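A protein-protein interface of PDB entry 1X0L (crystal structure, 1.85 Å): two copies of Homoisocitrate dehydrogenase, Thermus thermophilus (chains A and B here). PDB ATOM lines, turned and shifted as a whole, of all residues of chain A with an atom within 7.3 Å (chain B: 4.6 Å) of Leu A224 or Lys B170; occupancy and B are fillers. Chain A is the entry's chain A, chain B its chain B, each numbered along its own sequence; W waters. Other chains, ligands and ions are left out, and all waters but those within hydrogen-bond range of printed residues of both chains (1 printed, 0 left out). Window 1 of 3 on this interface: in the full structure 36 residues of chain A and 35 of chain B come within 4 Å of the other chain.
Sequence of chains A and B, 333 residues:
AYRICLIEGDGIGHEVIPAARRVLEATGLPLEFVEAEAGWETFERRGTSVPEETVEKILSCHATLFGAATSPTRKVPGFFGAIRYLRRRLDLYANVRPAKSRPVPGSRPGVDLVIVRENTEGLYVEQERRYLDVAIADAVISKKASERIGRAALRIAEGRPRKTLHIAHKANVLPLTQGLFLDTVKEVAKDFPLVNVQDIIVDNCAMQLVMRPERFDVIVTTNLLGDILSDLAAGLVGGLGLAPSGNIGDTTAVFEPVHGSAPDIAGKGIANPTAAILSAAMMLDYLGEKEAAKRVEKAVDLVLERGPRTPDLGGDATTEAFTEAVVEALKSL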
ATOM      1  N   ARG A 117      11.114   9.269  16.035  1.00  0.00           N
ATOM      2  CA  ARG A 117      10.209   8.352  15.353  1.00  0.00           C
ATOM      3  C   ARG A 117       9.823   7.275  16.350  1.00  0.00           C
ATOM      4  O   ARG A 117      10.541   7.025  17.312  1.00  0.00           O
ATOM      5  CB  ARG A 117      10.865   7.722  14.116  1.00  0.00           C
ATOM      6  CG  ARG A 117      11.919   6.670  14.402  1.00  0.00           C
ATOM      7  CD  ARG A 117      12.262   5.912  13.127  1.00  0.00           C
ATOM      8  NE  ARG A 117      13.266   4.872  13.323  1.00  0.00           N
ATOM      9  CZ  ARG A 117      13.074   3.742  14.000  1.00  0.00           C
ATOM     10  NH1 ARG A 117      14.062   2.865  14.110  1.00  0.00           N
ATOM     11  NH2 ARG A 117      11.902   3.481  14.561  1.00  0.00           N
ATOM     12  N   GLU A 118       8.688   6.633  16.132  1.00  0.00           N
ATOM     13  CA  GLU A 118       8.258   5.619  17.075  1.00  0.00           C
ATOM     14  C   GLU A 118       8.913   4.265  16.867  1.00  0.00           C
ATOM     15  O   GLU A 118       9.321   3.912  15.757  1.00  0.00           O
ATOM     16  CB  GLU A 118       6.737   5.432  16.991  1.00  0.00           C
ATOM     17  CG  GLU A 118       6.297   4.553  15.825  1.00  0.00           C
ATOM     18  CD  GLU A 118       4.786   4.468  15.672  1.00  0.00           C
ATOM     19  OE1 GLU A 118       4.237   5.125  14.758  1.00  0.00           O
ATOM     20  OE2 GLU A 118       4.152   3.751  16.468  1.00  0.00           O
ATOM     21  N   GLU A 126       4.812  -5.246  13.386  1.00  0.00           N
ATOM     22  CA  GLU A 126       4.229  -5.123  12.054  1.00  0.00           C
ATOM     23  C   GLU A 126       4.555  -6.415  11.311  1.00  0.00           C
ATOM     24  O   GLU A 126       5.716  -6.695  11.013  1.00  0.00           O
ATOM     25  CB  GLU A 126       4.816  -3.906  11.333  1.00  0.00           C
ATOM     26  CG  GLU A 126       4.655  -2.613  12.130  1.00  0.00           C
ATOM     27  CD  GLU A 126       5.228  -1.401  11.423  1.00  0.00           C
ATOM     28  OE1 GLU A 126       4.464  -0.705  10.723  1.00  0.00           O
ATOM     29  OE2 GLU A 126       6.446  -1.149  11.562  1.00  0.00           O
ATOM     30  N   GLU A 128       4.741  -9.493   8.438  1.00  0.00           N
ATOM     31  CA  GLU A 128       5.061  -9.743   7.037  1.00  0.00           C
ATOM     32  C   GLU A 128       4.516 -11.123   6.728  1.00  0.00           C
ATOM     33  O   GLU A 128       4.448 -11.981   7.607  1.00  0.00           O
ATOM     34  CB  GLU A 128       6.569  -9.811   6.796  1.00  0.00           C
ATOM     35  CG  GLU A 128       7.305  -8.516   6.694  1.00  0.00           C
ATOM     36  CD  GLU A 128       8.650  -8.724   6.025  1.00  0.00           C
ATOM     37  OE1 GLU A 128       8.816  -8.277   4.872  1.00  0.00           O
ATOM     38  OE2 GLU A 128       9.528  -9.361   6.640  1.00  0.00           O
ATOM     39  N   ASP A 138       3.091  -5.145   6.403  1.00  0.00           N
ATOM     40  CA  ASP A 138       2.166  -4.170   6.972  1.00  0.00           C
ATOM     41  C   ASP A 138       2.874  -2.921   7.498  1.00  0.00           C
ATOM     42  O   ASP A 138       3.851  -3.020   8.233  1.00  0.00           O
ATOM     43  CB  ASP A 138       1.388  -4.777   8.148  1.00  0.00           C
ATOM     44  CG  ASP A 138       0.318  -5.757   7.717  1.00  0.00           C
ATOM     45  OD1 ASP A 138       0.129  -5.948   6.500  1.00  0.00           O
ATOM     46  OD2 ASP A 138      -0.338  -6.336   8.611  1.00  0.00           O
ATOM     47  N   ALA A 139       2.376  -1.751   7.110  1.00  0.00           N
ATOM     48  CA  ALA A 139       2.897  -0.483   7.611  1.00  0.00           C
ATOM     49  C   ALA A 139       1.705  -0.057   8.457  1.00  0.00           C
ATOM     50  O   ALA A 139       0.642   0.247   7.917  1.00  0.00           O
ATOM     51  CB  ALA A 139       3.126   0.499   6.479  1.00  0.00           C
ATOM     52  N   VAL A 202       8.063  13.964   3.429  1.00  0.00           N
ATOM     53  CA  VAL A 202       9.378  13.396   3.716  1.00  0.00           C
ATOM     54  C   VAL A 202      10.409  13.534   2.597  1.00  0.00           C
ATOM     55  O   VAL A 202      11.587  13.797   2.859  1.00  0.00           O
ATOM     56  CB  VAL A 202       9.271  11.906   4.122  1.00  0.00           C
ATOM     57  CG1 VAL A 202       8.865  11.061   2.927  1.00  0.00           C
ATOM     58  CG2 VAL A 202      10.601  11.431   4.698  1.00  0.00           C
ATOM     59  N   THR A 221       8.613  11.801  12.689  1.00  0.00           N
ATOM     60  CA  THR A 221       8.174  11.069  11.512  1.00  0.00           C
ATOM     61  C   THR A 221       7.804   9.651  11.915  1.00  0.00           C
ATOM     62  O   THR A 221       7.826   9.317  13.100  1.00  0.00           O
ATOM     63  CB  THR A 221       9.300  11.047  10.451  1.00  0.00           C
ATOM     64  OG1 THR A 221       8.786  10.575   9.199  1.00  0.00           O
ATOM     65  CG2 THR A 221      10.440  10.147  10.909  1.00  0.00           C
ATOM     66  N   THR A 222       7.457   8.826  10.933  1.00  0.00           N
ATOM     67  CA  THR A 222       7.085   7.445  11.206  1.00  0.00           C
ATOM     68  C   THR A 222       8.276   6.496  11.062  1.00  0.00           C
ATOM     69  O   THR A 222       9.385   6.913  10.728  1.00  0.00           O
ATOM     70  CB  THR A 222       5.944   6.974  10.270  1.00  0.00           C
ATOM     71  OG1 THR A 222       6.352   7.116   8.907  1.00  0.00           O
ATOM     72  CG2 THR A 222       4.684   7.799  10.507  1.00  0.00           C
ATOM     73  N   ASN A 223       8.008   5.221  11.322  1.00  0.00           N
ATOM     74  CA  ASN A 223       8.978   4.126  11.288  1.00  0.00           C
ATOM     75  C   ASN A 223      10.171   4.235  10.332  1.00  0.00           C
ATOM     76  O   ASN A 223      11.219   4.801  10.674  1.00  0.00           O
ATOM     77  CB  ASN A 223       8.230   2.814  11.001  1.00  0.00           C
ATOM     78  CG  ASN A 223       8.873   1.613  11.665  1.00  0.00           C
ATOM     79  OD1 ASN A 223      10.067   1.349  11.493  1.00  0.00           O
ATOM     80  ND2 ASN A 223       8.076   0.866  12.425  1.00  0.00           N
ATOM     81  N   LEU A 224      10.010   3.666   9.142  1.00  0.00           N
ATOM     82  CA  LEU A 224      11.066   3.641   8.128  1.00  0.00           C
ATOM     83  C   LEU A 224      11.587   4.981   7.612  1.00  0.00           C
ATOM     84  O   LEU A 224      12.715   5.053   7.118  1.00  0.00           O
ATOM     85  CB  LEU A 224      10.617   2.788   6.933  1.00  0.00           C
ATOM     86  CG  LEU A 224      10.334   1.298   7.171  1.00  0.00           C
ATOM     87  CD1 LEU A 224      11.494   0.659   7.924  1.00  0.00           C
ATOM     88  CD2 LEU A 224       9.051   1.135   7.958  1.00  0.00           C
ATOM     89  N   LEU A 225      10.785   6.037   7.714  1.00  0.00           N
ATOM     90  CA  LEU A 225      11.221   7.346   7.235  1.00  0.00           C
ATOM     91  C   LEU A 225      12.266   7.938   8.177  1.00  0.00           C
ATOM     92  O   LEU A 225      13.263   8.514   7.739  1.00  0.00           O
ATOM     93  CB  LEU A 225      10.029   8.301   7.110  1.00  0.00           C
ATOM     94  CG  LEU A 225       8.895   7.877   6.166  1.00  0.00           C
ATOM     95  CD1 LEU A 225       7.808   8.941   6.173  1.00  0.00           C
ATOM     96  CD2 LEU A 225       9.428   7.675   4.750  1.00  0.00           C
ATOM     97  N   GLY A 226      12.037   7.787   9.475  1.00  0.00           N
ATOM     98  CA  GLY A 226      12.983   8.311  10.439  1.00  0.00           C
ATOM     99  C   GLY A 226      14.357   7.706  10.230  1.00  0.00           C
ATOM    100  O   GLY A 226      15.364   8.411  10.287  1.00  0.00           O
ATOM    101  N   ASP A 227      14.389   6.397   9.985  1.00  0.00           N
ATOM    102  CA  ASP A 227      15.648   5.683   9.776  1.00  0.00           C
ATOM    103  C   ASP A 227      16.508   6.341   8.711  1.00  0.00           C
ATOM    104  O   ASP A 227      17.663   6.702   8.955  1.00  0.00           O
ATOM    105  CB  ASP A 227      15.380   4.241   9.358  1.00  0.00           C
ATOM    106  CG  ASP A 227      14.551   3.489  10.364  1.00  0.00           C
ATOM    107  OD1 ASP A 227      14.918   3.499  11.558  1.00  0.00           O
ATOM    108  OD2 ASP A 227      13.538   2.880   9.959  1.00  0.00           O
ATOM    109  N   ILE A 228      15.944   6.499   7.525  1.00  0.00           N
ATOM    110  CA  ILE A 228      16.692   7.099   6.440  1.00  0.00           C
ATOM    111  C   ILE A 228      17.029   8.575   6.678  1.00  0.00           C
ATOM    112  O   ILE A 228      18.119   9.019   6.335  1.00  0.00           O
ATOM    113  CB  ILE A 228      15.947   6.911   5.095  1.00  0.00           C
ATOM    114  CG1 ILE A 228      16.784   7.481   3.950  1.00  0.00           C
ATOM    115  CG2 ILE A 228      14.586   7.564   5.158  1.00  0.00           C
ATOM    116  CD1 ILE A 228      16.451   6.873   2.600  1.00  0.00           C
ATOM    117  N   LEU A 229      16.121   9.337   7.282  1.00  0.00           N
ATOM    118  CA  LEU A 229      16.415  10.746   7.527  1.00  0.00           C
ATOM    119  C   LEU A 229      17.573  10.905   8.510  1.00  0.00           C
ATOM    120  O   LEU A 229      18.424  11.778   8.339  1.00  0.00           O
ATOM    121  CB  LEU A 229      15.183  11.483   8.059  1.00  0.00           C
ATOM    122  CG  LEU A 229      14.012  11.672   7.089  1.00  0.00           C
ATOM    123  CD1 LEU A 229      12.913  12.455   7.788  1.00  0.00           C
ATOM    124  CD2 LEU A 229      14.478  12.420   5.835  1.00  0.00           C
ATOM    125  N   HIS B 169      18.412  -2.147  -0.200  1.00  0.00           N
ATOM    126  CA  HIS B 169      17.299  -2.862   0.408  1.00  0.00           C
ATOM    127  C   HIS B 169      17.179  -2.666   1.914  1.00  0.00           C
ATOM    128  O   HIS B 169      18.008  -2.016   2.550  1.00  0.00           O
ATOM    129  CB  HIS B 169      17.471  -4.354   0.150  1.00  0.00           C
ATOM    130  CG  HIS B 169      18.643  -4.937   0.869  1.00  0.00           C
ATOM    131  ND1 HIS B 169      19.936  -4.802   0.414  1.00  0.00           N
ATOM    132  CD2 HIS B 169      18.728  -5.578   2.057  1.00  0.00           C
ATOM    133  CE1 HIS B 169      20.768  -5.336   1.290  1.00  0.00           C
ATOM    134  NE2 HIS B 169      20.060  -5.814   2.298  1.00  0.00           N
ATOM    135  N   LYS B 170      16.145  -3.283   2.475  1.00  0.00           N
ATOM    136  CA  LYS B 170      15.871  -3.226   3.906  1.00  0.00           C
ATOM    137  C   LYS B 170      15.563  -4.658   4.364  1.00  0.00           C
ATOM    138  O   LYS B 170      14.706  -4.883   5.226  1.00  0.00           O
ATOM    139  CB  LYS B 170      14.658  -2.322   4.146  1.00  0.00           C
ATOM    140  CG  LYS B 170      14.415  -1.923   5.579  1.00  0.00           C
ATOM    141  CD  LYS B 170      15.104  -0.612   5.923  1.00  0.00           C
ATOM    142  CE  LYS B 170      14.753  -0.182   7.336  1.00  0.00           C
ATOM    143  NZ  LYS B 170      15.379   1.108   7.706  1.00  0.00           N
ATOM    144  N   ALA B 171      16.261  -5.627   3.778  1.00  0.00           N
ATOM    145  CA  ALA B 171      16.039  -7.032   4.103  1.00  0.00           C
ATOM    146  C   ALA B 171      16.410  -7.370   5.538  1.00  0.00           C
ATOM    147  O   ALA B 171      15.971  -8.384   6.074  1.00  0.00           O
ATOM    148  CB  ALA B 171      16.817  -7.924   3.140  1.00  0.00           C
ATOM    149  N   ASN B 172      17.215  -6.517   6.161  1.00  0.00           N
ATOM    150  CA  ASN B 172      17.628  -6.742   7.536  1.00  0.00           C
ATOM    151  C   ASN B 172      16.436  -6.673   8.489  1.00  0.00           C
ATOM    152  O   ASN B 172      16.374  -7.418   9.465  1.00  0.00           O
ATOM    153  CB  ASN B 172      18.695  -5.717   7.942  1.00  0.00           C
ATOM    154  CG  ASN B 172      18.198  -4.284   7.862  1.00  0.00           C
ATOM    155  OD1 ASN B 172      17.630  -3.861   6.854  1.00  0.00           O
ATOM    156  ND2 ASN B 172      18.425  -3.523   8.928  1.00  0.00           N
ATOM    157  N   VAL B 173      15.480  -5.793   8.202  1.00  0.00           N
ATOM    158  CA  VAL B 173      14.313  -5.667   9.071  1.00  0.00           C
ATOM    159  C   VAL B 173      13.036  -6.209   8.433  1.00  0.00           C
ATOM    160  O   VAL B 173      12.058  -6.481   9.124  1.00  0.00           O
ATOM    161  CB  VAL B 173      14.092  -4.202   9.502  1.00  0.00           C
ATOM    162  CG1 VAL B 173      15.377  -3.640  10.088  1.00  0.00           C
ATOM    163  CG2 VAL B 173      13.636  -3.369   8.332  1.00  0.00           C
ATOM    164  N   LEU B 174      13.050  -6.366   7.114  1.00  0.00           N
ATOM    165  CA  LEU B 174      11.897  -6.897   6.392  1.00  0.00           C
ATOM    166  C   LEU B 174      12.378  -8.050   5.519  1.00  0.00           C
ATOM    167  O   LEU B 174      12.404  -7.952   4.293  1.00  0.00           O
ATOM    168  CB  LEU B 174      11.254  -5.800   5.540  1.00  0.00           C
ATOM    169  CG  LEU B 174      10.600  -4.672   6.343  1.00  0.00           C
ATOM    170  CD1 LEU B 174      10.253  -3.512   5.425  1.00  0.00           C
ATOM    171  CD2 LEU B 174       9.348  -5.206   7.043  1.00  0.00           C
ATOM    172  N   GLN B 178      11.506  -7.418   1.481  1.00  0.00           N
ATOM    173  CA  GLN B 178      12.782  -6.908   0.997  1.00  0.00           C
ATOM    174  C   GLN B 178      13.763  -8.030   0.668  1.00  0.00           C
ATOM    175  O   GLN B 178      14.608  -7.883  -0.218  1.00  0.00           O
ATOM    176  CB  GLN B 178      13.382  -5.952   2.026  1.00  0.00           C
ATOM    177  CG  GLN B 178      12.638  -4.622   2.137  1.00  0.00           C
ATOM    178  CD  GLN B 178      12.850  -3.724   0.928  1.00  0.00           C
ATOM    179  OE1 GLN B 178      13.988  -3.428   0.550  1.00  0.00           O
ATOM    180  NE2 GLN B 178      11.754  -3.271   0.325  1.00  0.00           N
ATOM    181  N   VAL B 202      19.431   0.349   2.661  1.00  0.00           N
ATOM    182  CA  VAL B 202      19.005   1.665   2.207  1.00  0.00           C
ATOM    183  C   VAL B 202      19.437   2.821   3.110  1.00  0.00           C
ATOM    184  O   VAL B 202      19.787   3.894   2.620  1.00  0.00           O
ATOM    185  CB  VAL B 202      17.470   1.717   2.021  1.00  0.00           C
ATOM    186  CG1 VAL B 202      16.776   1.493   3.356  1.00  0.00           C
ATOM    187  CG2 VAL B 202      17.066   3.049   1.411  1.00  0.00           C
ATOM    188  N   ASP B 203      19.425   2.609   4.421  1.00  0.00           N
ATOM    189  CA  ASP B 203      19.819   3.676   5.334  1.00  0.00           C
ATOM    190  C   ASP B 203      21.284   4.040   5.118  1.00  0.00           C
ATOM    191  O   ASP B 203      21.641   5.217   5.065  1.00  0.00           O
ATOM    192  CB  ASP B 203      19.576   3.245   6.780  1.00  0.00           C
ATOM    193  CG  ASP B 203      18.124   2.895   7.038  1.00  0.00           C
ATOM    194  OD1 ASP B 203      17.249   3.758   6.798  1.00  0.00           O
ATOM    195  OD2 ASP B 203      17.855   1.758   7.475  1.00  0.00           O
HETATM  196  O   HOH W   1      14.266   2.953   6.122  1.00  0.00           O
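The side-chain amino group of Lys B170 is in salt-bridge range of the side-chain carboxylate of Asp A227 (3.4 Å). The side-chain carboxylate (OD1) of Asp B203 lies within hydrogen-bond range of the backbone NH (N) of Ile A228 (3.1 Å).
The guanidinium group (NH1) of Arg A117 is in salt-bridge range of the side-chain carboxylate (OD1) of Asp A227, at 2.8 Å. The backbone carbonyl oxygen of Lys B170 lies close to the side-chain amide oxygen of Asn B172 (3.5 Å). The backbone NH of Lys B170 is in hydrogen-bond range of the side-chain amide oxygen of Gln B178. NZ of Lys B170 is in salt-bridge range of OD2 of Asp B203, at 2.6 Å.
Leu B174 touches Glu A128. CD1 of Leu A224 touches CE of Lys B170, 3.4 Å away. CB of Asp A227 touches OD1 of Asp B203, 3.2 Å away.
Of the printed residues of chain B, Glu A128 touches Leu B174. Ala A139 touches none of the printed residues of chain B. Printed residues of chain B within 4 Å of Leu A224: Lys B170. Of the printed residues of chain B, Asp A227 touches Lys B170 and Asp B203. Of the printed residues of chain B, Ile A228 touches Asp B203. Leu A229 touches none of the printed residues of chain B. Lys B170 touches two residues of chain A. Of the printed residues of chain A, Leu B174 touches Glu A128 (3.3 Å). Printed residues of chain A within 4 Å of Asp B203: Asp A227 (3.2 Å) and Ile A228 (3.1 Å). The nearest residue of chain A that does not touch Lys B170 is Ile A228 (5.4 Å).
1 position is printed for both chains.
Water W1 lies within hydrogen-bond range of the side-chain amino group of Lys B170, the backbone carbonyl oxygen of Leu A224 and the side-chain carboxylate of Asp B203.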
